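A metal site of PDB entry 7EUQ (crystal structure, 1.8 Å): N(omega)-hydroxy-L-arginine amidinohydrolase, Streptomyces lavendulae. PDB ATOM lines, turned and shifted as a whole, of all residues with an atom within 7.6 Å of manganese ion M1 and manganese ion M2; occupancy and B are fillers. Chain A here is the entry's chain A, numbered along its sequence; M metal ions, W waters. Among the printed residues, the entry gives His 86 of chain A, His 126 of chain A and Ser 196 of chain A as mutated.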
ATOM      1  N   THR A  85     -20.000 -37.312  -5.282  1.00  0.00           N
ATOM      2  CA  THR A  85     -21.278 -36.569  -5.150  1.00  0.00           C
ATOM      3  C   THR A  85     -21.816 -36.658  -3.725  1.00  0.00           C
ATOM      4  O   THR A  85     -21.569 -37.671  -3.023  1.00  0.00           O
ATOM      5  CB  THR A  85     -22.314 -37.085  -6.147  1.00  0.00           C
ATOM      6  OG1 THR A  85     -23.408 -36.155  -6.139  1.00  0.00           O
ATOM      7  CG2 THR A  85     -22.803 -38.460  -5.798  1.00  0.00           C
ATOM      8  N   HIS A  86     -22.655 -35.704  -3.344  1.00  0.00           N
ATOM      9  CA  HIS A  86     -23.352 -35.718  -2.034  1.00  0.00           C
ATOM     10  C   HIS A  86     -24.263 -36.936  -1.957  1.00  0.00           C
ATOM     11  O   HIS A  86     -24.519 -37.408  -0.862  1.00  0.00           O
ATOM     12  CB  HIS A  86     -24.149 -34.437  -1.756  1.00  0.00           C
ATOM     13  CG  HIS A  86     -24.100 -34.067  -0.309  1.00  0.00           C
ATOM     14  ND1 HIS A  86     -24.551 -32.856   0.159  1.00  0.00           N
ATOM     15  CD2 HIS A  86     -23.589 -34.723   0.761  1.00  0.00           C
ATOM     16  CE1 HIS A  86     -24.359 -32.817   1.456  1.00  0.00           C
ATOM     17  NE2 HIS A  86     -23.767 -33.933   1.856  1.00  0.00           N
ATOM     18  N   SER A  87     -24.722 -37.460  -3.086  1.00  0.00           N
ATOM     19  CA  SER A  87     -25.709 -38.553  -3.152  1.00  0.00           C
ATOM     20  C   SER A  87     -25.162 -39.832  -2.501  1.00  0.00           C
ATOM     21  O   SER A  87     -25.969 -40.679  -2.117  1.00  0.00           O
ATOM     22  CB  SER A  87     -26.152 -38.775  -4.575  1.00  0.00           C
ATOM     23  OG  SER A  87     -27.017 -37.743  -4.974  1.00  0.00           O
ATOM     24  N   TYR A 107     -24.853 -31.388   8.557  1.00  0.00           N
ATOM     25  CA  TYR A 107     -25.029 -31.469   7.095  1.00  0.00           C
ATOM     26  C   TYR A 107     -24.738 -30.086   6.545  1.00  0.00           C
ATOM     27  O   TYR A 107     -25.624 -29.185   6.577  1.00  0.00           O
ATOM     28  CB  TYR A 107     -26.405 -32.031   6.757  1.00  0.00           C
ATOM     29  CG  TYR A 107     -26.600 -32.517   5.347  1.00  0.00           C
ATOM     30  CD1 TYR A 107     -26.973 -31.652   4.327  1.00  0.00           C
ATOM     31  CD2 TYR A 107     -26.515 -33.863   5.054  1.00  0.00           C
ATOM     32  CE1 TYR A 107     -27.206 -32.122   3.041  1.00  0.00           C
ATOM     33  CE2 TYR A 107     -26.763 -34.347   3.777  1.00  0.00           C
ATOM     34  CZ  TYR A 107     -27.066 -33.471   2.763  1.00  0.00           C
ATOM     35  OH  TYR A 107     -27.317 -34.007   1.528  1.00  0.00           O
ATOM     36  N   ILE A 108     -23.481 -29.908   6.135  1.00  0.00           N
ATOM     37  CA  ILE A 108     -22.914 -28.582   5.816  1.00  0.00           C
ATOM     38  C   ILE A 108     -23.103 -28.388   4.309  1.00  0.00           C
ATOM     39  O   ILE A 108     -22.372 -29.020   3.519  1.00  0.00           O
ATOM     40  CB  ILE A 108     -21.463 -28.434   6.280  1.00  0.00           C
ATOM     41  CG1 ILE A 108     -21.276 -28.810   7.760  1.00  0.00           C
ATOM     42  CG2 ILE A 108     -20.983 -27.030   5.979  1.00  0.00           C
ATOM     43  CD1 ILE A 108     -19.889 -28.525   8.281  1.00  0.00           C
ATOM     44  N   ASP A 109     -23.991 -27.483   3.937  1.00  0.00           N
ATOM     45  CA  ASP A 109     -24.518 -27.415   2.555  1.00  0.00           C
ATOM     46  C   ASP A 109     -25.182 -26.056   2.310  1.00  0.00           C
ATOM     47  O   ASP A 109     -25.817 -25.541   3.254  1.00  0.00           O
ATOM     48  CB  ASP A 109     -25.537 -28.549   2.419  1.00  0.00           C
ATOM     49  CG  ASP A 109     -25.778 -28.991   0.996  1.00  0.00           C
ATOM     50  OD1 ASP A 109     -25.961 -28.114   0.121  1.00  0.00           O
ATOM     51  OD2 ASP A 109     -25.721 -30.219   0.777  1.00  0.00           O
ATOM     52  N   GLY A 110     -25.112 -25.594   1.079  1.00  0.00           N
ATOM     53  CA  GLY A 110     -25.792 -24.373   0.602  1.00  0.00           C
ATOM     54  C   GLY A 110     -27.296 -24.588   0.452  1.00  0.00           C
ATOM     55  O   GLY A 110     -28.010 -23.578   0.340  1.00  0.00           O
ATOM     56  N   HIS A 111     -27.744 -25.847   0.420  1.00  0.00           N
ATOM     57  CA  HIS A 111     -29.148 -26.260   0.152  1.00  0.00           C
ATOM     58  C   HIS A 111     -29.659 -27.137   1.295  1.00  0.00           C
ATOM     59  O   HIS A 111     -28.869 -27.464   2.196  1.00  0.00           O
ATOM     60  CB  HIS A 111     -29.229 -27.015  -1.192  1.00  0.00           C
ATOM     61  CG  HIS A 111     -28.608 -26.308  -2.345  1.00  0.00           C
ATOM     62  ND1 HIS A 111     -27.287 -26.536  -2.727  1.00  0.00           N
ATOM     63  CD2 HIS A 111     -29.117 -25.422  -3.220  1.00  0.00           C
ATOM     64  CE1 HIS A 111     -27.014 -25.781  -3.769  1.00  0.00           C
ATOM     65  NE2 HIS A 111     -28.121 -25.070  -4.078  1.00  0.00           N
ATOM     66  N   GLY A 112     -30.949 -27.514   1.282  1.00  0.00           N
ATOM     67  CA  GLY A 112     -31.478 -28.435   2.290  1.00  0.00           C
ATOM     68  C   GLY A 112     -31.354 -29.907   1.907  1.00  0.00           C
ATOM     69  O   GLY A 112     -31.427 -30.730   2.830  1.00  0.00           O
ATOM     70  N   ASP A 113     -31.292 -30.223   0.622  1.00  0.00           N
ATOM     71  CA  ASP A 113     -31.280 -31.608   0.109  1.00  0.00           C
ATOM     72  C   ASP A 113     -32.424 -32.376   0.758  1.00  0.00           C
ATOM     73  O   ASP A 113     -32.235 -33.547   1.116  1.00  0.00           O
ATOM     74  CB  ASP A 113     -29.922 -32.274   0.294  1.00  0.00           C
ATOM     75  CG  ASP A 113     -28.806 -31.609  -0.479  1.00  0.00           C
ATOM     76  OD1 ASP A 113     -29.089 -30.693  -1.255  1.00  0.00           O
ATOM     77  OD2 ASP A 113     -27.661 -32.078  -0.344  1.00  0.00           O
ATOM     78  N   HIS A 126     -29.636 -35.515  -5.870  1.00  0.00           N
ATOM     79  CA  HIS A 126     -28.842 -34.731  -4.900  1.00  0.00           C
ATOM     80  C   HIS A 126     -29.793 -33.948  -3.988  1.00  0.00           C
ATOM     81  O   HIS A 126     -29.598 -33.958  -2.781  1.00  0.00           O
ATOM     82  CB  HIS A 126     -27.821 -33.826  -5.631  1.00  0.00           C
ATOM     83  CG  HIS A 126     -26.905 -33.088  -4.715  1.00  0.00           C
ATOM     84  ND1 HIS A 126     -25.907 -32.263  -5.182  1.00  0.00           N
ATOM     85  CD2 HIS A 126     -26.831 -33.048  -3.363  1.00  0.00           C
ATOM     86  CE1 HIS A 126     -25.254 -31.752  -4.185  1.00  0.00           C
ATOM     87  NE2 HIS A 126     -25.817 -32.198  -3.045  1.00  0.00           N
ATOM     88  N   GLY A 127     -30.844 -33.346  -4.537  1.00  0.00           N
ATOM     89  CA  GLY A 127     -31.791 -32.554  -3.743  1.00  0.00           C
ATOM     90  C   GLY A 127     -32.618 -33.380  -2.784  1.00  0.00           C
ATOM     91  O   GLY A 127     -33.544 -32.802  -2.177  1.00  0.00           O
ATOM     92  N   VAL A 129     -31.234 -36.143  -0.760  1.00  0.00           N
ATOM     93  CA  VAL A 129     -30.305 -37.011   0.013  1.00  0.00           C
ATOM     94  C   VAL A 129     -30.678 -37.009   1.484  1.00  0.00           C
ATOM     95  O   VAL A 129     -30.811 -38.124   2.043  1.00  0.00           O
ATOM     96  CB  VAL A 129     -28.840 -36.592  -0.194  1.00  0.00           C
ATOM     97  CG1 VAL A 129     -27.946 -37.318   0.803  1.00  0.00           C
ATOM     98  CG2 VAL A 129     -28.418 -36.803  -1.614  1.00  0.00           C
ATOM     99  N   LEU A 130     -30.830 -35.847   2.122  1.00  0.00           N
ATOM    100  CA  LEU A 130     -31.027 -35.783   3.591  1.00  0.00           C
ATOM    101  C   LEU A 130     -32.424 -36.292   3.941  1.00  0.00           C
ATOM    102  O   LEU A 130     -32.537 -37.022   4.912  1.00  0.00           O
ATOM    103  CB  LEU A 130     -30.806 -34.361   4.117  1.00  0.00           C
ATOM    104  CG  LEU A 130     -30.872 -34.183   5.639  1.00  0.00           C
ATOM    105  CD1 LEU A 130     -29.992 -35.188   6.372  1.00  0.00           C
ATOM    106  CD2 LEU A 130     -30.504 -32.745   6.010  1.00  0.00           C
ATOM    107  N   ARG A 156     -28.867 -21.692   2.415  1.00  0.00           N
ATOM    108  CA  ARG A 156     -29.424 -20.363   2.076  1.00  0.00           C
ATOM    109  C   ARG A 156     -30.389 -20.422   0.888  1.00  0.00           C
ATOM    110  O   ARG A 156     -31.025 -19.393   0.625  1.00  0.00           O
ATOM    111  CB  ARG A 156     -28.300 -19.408   1.709  1.00  0.00           C
ATOM    112  CG  ARG A 156     -27.427 -19.944   0.585  1.00  0.00           C
ATOM    113  CD  ARG A 156     -26.069 -19.314   0.683  1.00  0.00           C
ATOM    114  NE  ARG A 156     -25.110 -19.911  -0.218  1.00  0.00           N
ATOM    115  CZ  ARG A 156     -24.156 -20.788   0.137  1.00  0.00           C
ATOM    116  NH1 ARG A 156     -24.014 -21.186   1.413  1.00  0.00           N
ATOM    117  NH2 ARG A 156     -23.322 -21.193  -0.805  1.00  0.00           N
ATOM    118  N   ASP A 157     -30.484 -21.564   0.226  1.00  0.00           N
ATOM    119  CA  ASP A 157     -31.329 -21.756  -0.983  1.00  0.00           C
ATOM    120  C   ASP A 157     -32.249 -22.956  -0.706  1.00  0.00           C
ATOM    121  O   ASP A 157     -31.880 -24.081  -1.079  1.00  0.00           O
ATOM    122  CB  ASP A 157     -30.423 -21.907  -2.211  1.00  0.00           C
ATOM    123  CG  ASP A 157     -31.138 -21.863  -3.553  1.00  0.00           C
ATOM    124  OD1 ASP A 157     -32.379 -21.718  -3.554  1.00  0.00           O
ATOM    125  OD2 ASP A 157     -30.440 -21.984  -4.573  1.00  0.00           O
ATOM    126  N   SER A 196     -20.923 -33.961   7.298  1.00  0.00           N
ATOM    127  CA  SER A 196     -21.127 -34.215   5.846  1.00  0.00           C
ATOM    128  C   SER A 196     -21.057 -32.908   5.084  1.00  0.00           C
ATOM    129  O   SER A 196     -21.956 -32.100   5.271  1.00  0.00           O
ATOM    130  CB  SER A 196     -22.399 -34.961   5.595  1.00  0.00           C
ATOM    131  OG  SER A 196     -22.552 -35.274   4.224  1.00  0.00           O
ATOM    132  N   ILE A 197     -20.003 -32.682   4.310  1.00  0.00           N
ATOM    133  CA  ILE A 197     -19.802 -31.377   3.613  1.00  0.00           C
ATOM    134  C   ILE A 197     -20.106 -31.504   2.112  1.00  0.00           C
ATOM    135  O   ILE A 197     -19.593 -32.427   1.428  1.00  0.00           O
ATOM    136  CB  ILE A 197     -18.392 -30.798   3.859  1.00  0.00           C
ATOM    137  CG1 ILE A 197     -18.150 -30.485   5.330  1.00  0.00           C
ATOM    138  CG2 ILE A 197     -18.201 -29.556   3.012  1.00  0.00           C
ATOM    139  CD1 ILE A 197     -16.721 -30.107   5.656  1.00  0.00           C
ATOM    140  N   ASP A 198     -20.856 -30.530   1.608  1.00  0.00           N
ATOM    141  CA  ASP A 198     -21.025 -30.213   0.170  1.00  0.00           C
ATOM    142  C   ASP A 198     -20.308 -28.872  -0.040  1.00  0.00           C
ATOM    143  O   ASP A 198     -20.735 -27.891   0.565  1.00  0.00           O
ATOM    144  CB  ASP A 198     -22.522 -30.212  -0.168  1.00  0.00           C
ATOM    145  CG  ASP A 198     -22.911 -29.735  -1.566  1.00  0.00           C
ATOM    146  OD1 ASP A 198     -22.026 -29.274  -2.290  1.00  0.00           O
ATOM    147  OD2 ASP A 198     -24.107 -29.815  -1.882  1.00  0.00           O
ATOM    148  N   TRP A 199     -19.223 -28.840  -0.811  1.00  0.00           N
ATOM    149  CA  TRP A 199     -18.428 -27.605  -1.032  1.00  0.00           C
ATOM    150  C   TRP A 199     -19.267 -26.488  -1.673  1.00  0.00           C
ATOM    151  O   TRP A 199     -18.817 -25.379  -1.592  1.00  0.00           O
ATOM    152  CB  TRP A 199     -17.187 -27.859  -1.897  1.00  0.00           C
ATOM    153  CG  TRP A 199     -16.268 -28.848  -1.292  1.00  0.00           C
ATOM    154  CD1 TRP A 199     -15.824 -30.023  -1.829  1.00  0.00           C
ATOM    155  CD2 TRP A 199     -15.672 -28.765   0.012  1.00  0.00           C
ATOM    156  NE1 TRP A 199     -15.006 -30.680  -0.946  1.00  0.00           N
ATOM    157  CE2 TRP A 199     -14.873 -29.917   0.183  1.00  0.00           C
ATOM    158  CE3 TRP A 199     -15.731 -27.828   1.036  1.00  0.00           C
ATOM    159  CZ2 TRP A 199     -14.184 -30.173   1.365  1.00  0.00           C
ATOM    160  CZ3 TRP A 199     -15.007 -28.050   2.184  1.00  0.00           C
ATOM    161  CH2 TRP A 199     -14.246 -29.215   2.342  1.00  0.00           C
ATOM    162  N   ASP A 200     -20.463 -26.732  -2.215  1.00  0.00           N
ATOM    163  CA  ASP A 200     -21.311 -25.608  -2.690  1.00  0.00           C
ATOM    164  C   ASP A 200     -21.752 -24.726  -1.501  1.00  0.00           C
ATOM    165  O   ASP A 200     -22.324 -23.634  -1.771  1.00  0.00           O
ATOM    166  CB  ASP A 200     -22.434 -26.044  -3.623  1.00  0.00           C
ATOM    167  CG  ASP A 200     -23.646 -26.687  -2.960  1.00  0.00           C
ATOM    168  OD1 ASP A 200     -23.858 -26.487  -1.716  1.00  0.00           O
ATOM    169  OD2 ASP A 200     -24.328 -27.479  -3.681  1.00  0.00           O
ATOM    170  N   VAL A 201     -21.465 -25.103  -0.251  1.00  0.00           N
ATOM    171  CA  VAL A 201     -21.780 -24.255   0.928  1.00  0.00           C
ATOM    172  C   VAL A 201     -20.932 -22.983   0.893  1.00  0.00           C
ATOM    173  O   VAL A 201     -21.346 -21.950   1.428  1.00  0.00           O
ATOM    174  CB  VAL A 201     -21.567 -24.999   2.258  1.00  0.00           C
ATOM    175  CG1 VAL A 201     -20.097 -25.230   2.565  1.00  0.00           C
ATOM    176  CG2 VAL A 201     -22.263 -24.280   3.389  1.00  0.00           C
ATOM    177  N   ALA A 209     -17.994 -26.464  -7.391  1.00  0.00           N
ATOM    178  CA  ALA A 209     -18.957 -27.594  -7.259  1.00  0.00           C
ATOM    179  C   ALA A 209     -19.854 -27.618  -8.513  1.00  0.00           C
ATOM    180  O   ALA A 209     -19.416 -27.136  -9.597  1.00  0.00           O
ATOM    181  CB  ALA A 209     -19.737 -27.446  -5.975  1.00  0.00           C
ATOM    182  N   TYR A 211     -23.304 -26.548  -8.171  1.00  0.00           N
ATOM    183  CA  TYR A 211     -24.212 -25.418  -7.897  1.00  0.00           C
ATOM    184  C   TYR A 211     -23.397 -24.209  -7.398  1.00  0.00           C
ATOM    185  O   TYR A 211     -22.400 -24.380  -6.666  1.00  0.00           O
ATOM    186  CB  TYR A 211     -25.317 -25.856  -6.934  1.00  0.00           C
ATOM    187  CG  TYR A 211     -26.325 -26.754  -7.597  1.00  0.00           C
ATOM    188  CD1 TYR A 211     -26.138 -28.128  -7.644  1.00  0.00           C
ATOM    189  CD2 TYR A 211     -27.418 -26.224  -8.253  1.00  0.00           C
ATOM    190  CE1 TYR A 211     -27.036 -28.960  -8.296  1.00  0.00           C
ATOM    191  CE2 TYR A 211     -28.333 -27.040  -8.908  1.00  0.00           C
ATOM    192  CZ  TYR A 211     -28.145 -28.409  -8.934  1.00  0.00           C
ATOM    193  OH  TYR A 211     -29.048 -29.214  -9.574  1.00  0.00           O
ATOM    194  N   VAL A 213     -24.283 -20.583  -5.565  1.00  0.00           N
ATOM    195  CA  VAL A 213     -25.335 -19.812  -4.813  1.00  0.00           C
ATOM    196  C   VAL A 213     -24.646 -18.777  -3.925  1.00  0.00           C
ATOM    197  O   VAL A 213     -23.819 -19.121  -3.078  1.00  0.00           O
ATOM    198  CB  VAL A 213     -26.286 -20.763  -4.048  1.00  0.00           C
ATOM    199  CG1 VAL A 213     -25.527 -21.850  -3.283  1.00  0.00           C
ATOM    200  CG2 VAL A 213     -27.254 -20.017  -3.134  1.00  0.00           C
ATOM    201  N   ALA A 240     -17.704 -33.841  -0.184  1.00  0.00           N
ATOM    202  CA  ALA A 240     -18.383 -34.120  -1.467  1.00  0.00           C
ATOM    203  C   ALA A 240     -18.425 -32.869  -2.322  1.00  0.00           C
ATOM    204  O   ALA A 240     -18.417 -31.794  -1.766  1.00  0.00           O
ATOM    205  CB  ALA A 240     -19.777 -34.650  -1.186  1.00  0.00           C
ATOM    206  N   GLU A 241     -18.517 -33.080  -3.646  1.00  0.00           N
ATOM    207  CA  GLU A 241     -18.934 -32.074  -4.644  1.00  0.00           C
ATOM    208  C   GLU A 241     -17.775 -31.127  -4.961  1.00  0.00           C
ATOM    209  O   GLU A 241     -18.046 -29.959  -5.191  1.00  0.00           O
ATOM    210  CB  GLU A 241     -20.186 -31.332  -4.179  1.00  0.00           C
ATOM    211  CG  GLU A 241     -21.363 -32.278  -3.921  1.00  0.00           C
ATOM    212  CD  GLU A 241     -22.230 -32.554  -5.144  1.00  0.00           C
ATOM    213  OE1 GLU A 241     -22.441 -31.605  -5.952  1.00  0.00           O
ATOM    214  OE2 GLU A 241     -22.722 -33.705  -5.266  1.00  0.00           O
HETATM  215 MN    MN M   1     -25.680 -28.166  -2.044  1.00  0.00          MN
HETATM  216 MN    MN M   2     -25.689 -31.342  -1.068  1.00  0.00          MN
HETATM  217  O   HOH W   1     -26.871 -29.687  -2.204  1.00  0.00           O
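Within 4 Å of manganese ion M2: His 86, Asp 109, Asp 113, His 126 and Asp 198. Along chain A the residues within 4 Å of manganese ion M2 span positions 86 to 198.
Manganese ion M2 is bound by a ring nitrogen (NE2) of His 126 (2.2 Å), the side-chain carboxylate (OD2) of Asp 109 (2.2 Å), the side-chain carboxylate (OD2) of Asp 113 (2.2 Å), a ring nitrogen (ND1) of His 86 (2.3 Å), water W1 (2.3 Å) and the side-chain carboxylate (OD2) of Asp 198 (2.3 Å).
A ring nitrogen (ND1) of His 126 lies close to the side-chain carboxylate of Glu 241, at 3.5 Å. The side-chain carboxylate (OD2) of Asp 113 lies close to the side-chain hydroxyl (OH) of Tyr 107. N of Val 129 is in hydrogen-bond range of O of Asp 113 (3.4 Å). The backbone NH (N) of Leu 130 is in hydrogen-bond range of the backbone carbonyl oxygen (O) of Asp 113. The backbone NH of Gly 110 lies close to the side-chain carboxylate of Asp 200, at 3.2 Å. O of Asp 200 sits at hydrogen-bond distance from NH2 of Arg 156 (2.8 Å). The backbone NH (N) of His 86 lies within hydrogen-bond range of the side-chain carboxylate (OE2) of Glu 241. The backbone NH (N) of Asp 198 sits at hydrogen-bond distance from the backbone carbonyl oxygen (O) of Ile 108 (2.9 Å).
Water W1 is bound to manganese ion M1 (1.9 Å). Manganese ion M1 is bound by the side-chain carboxylate (OD1) of Asp 109 (2.2 Å). OD2 of Asp 200 is bound to manganese ion M1 (2.2 Å). OD2 of Asp 198 binds manganese ion M1 (2.3 Å). ND1 of His 111 binds manganese ion M1, at 2.4 Å. OD1 of Asp 200 binds manganese ion M1 (2.5 Å).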
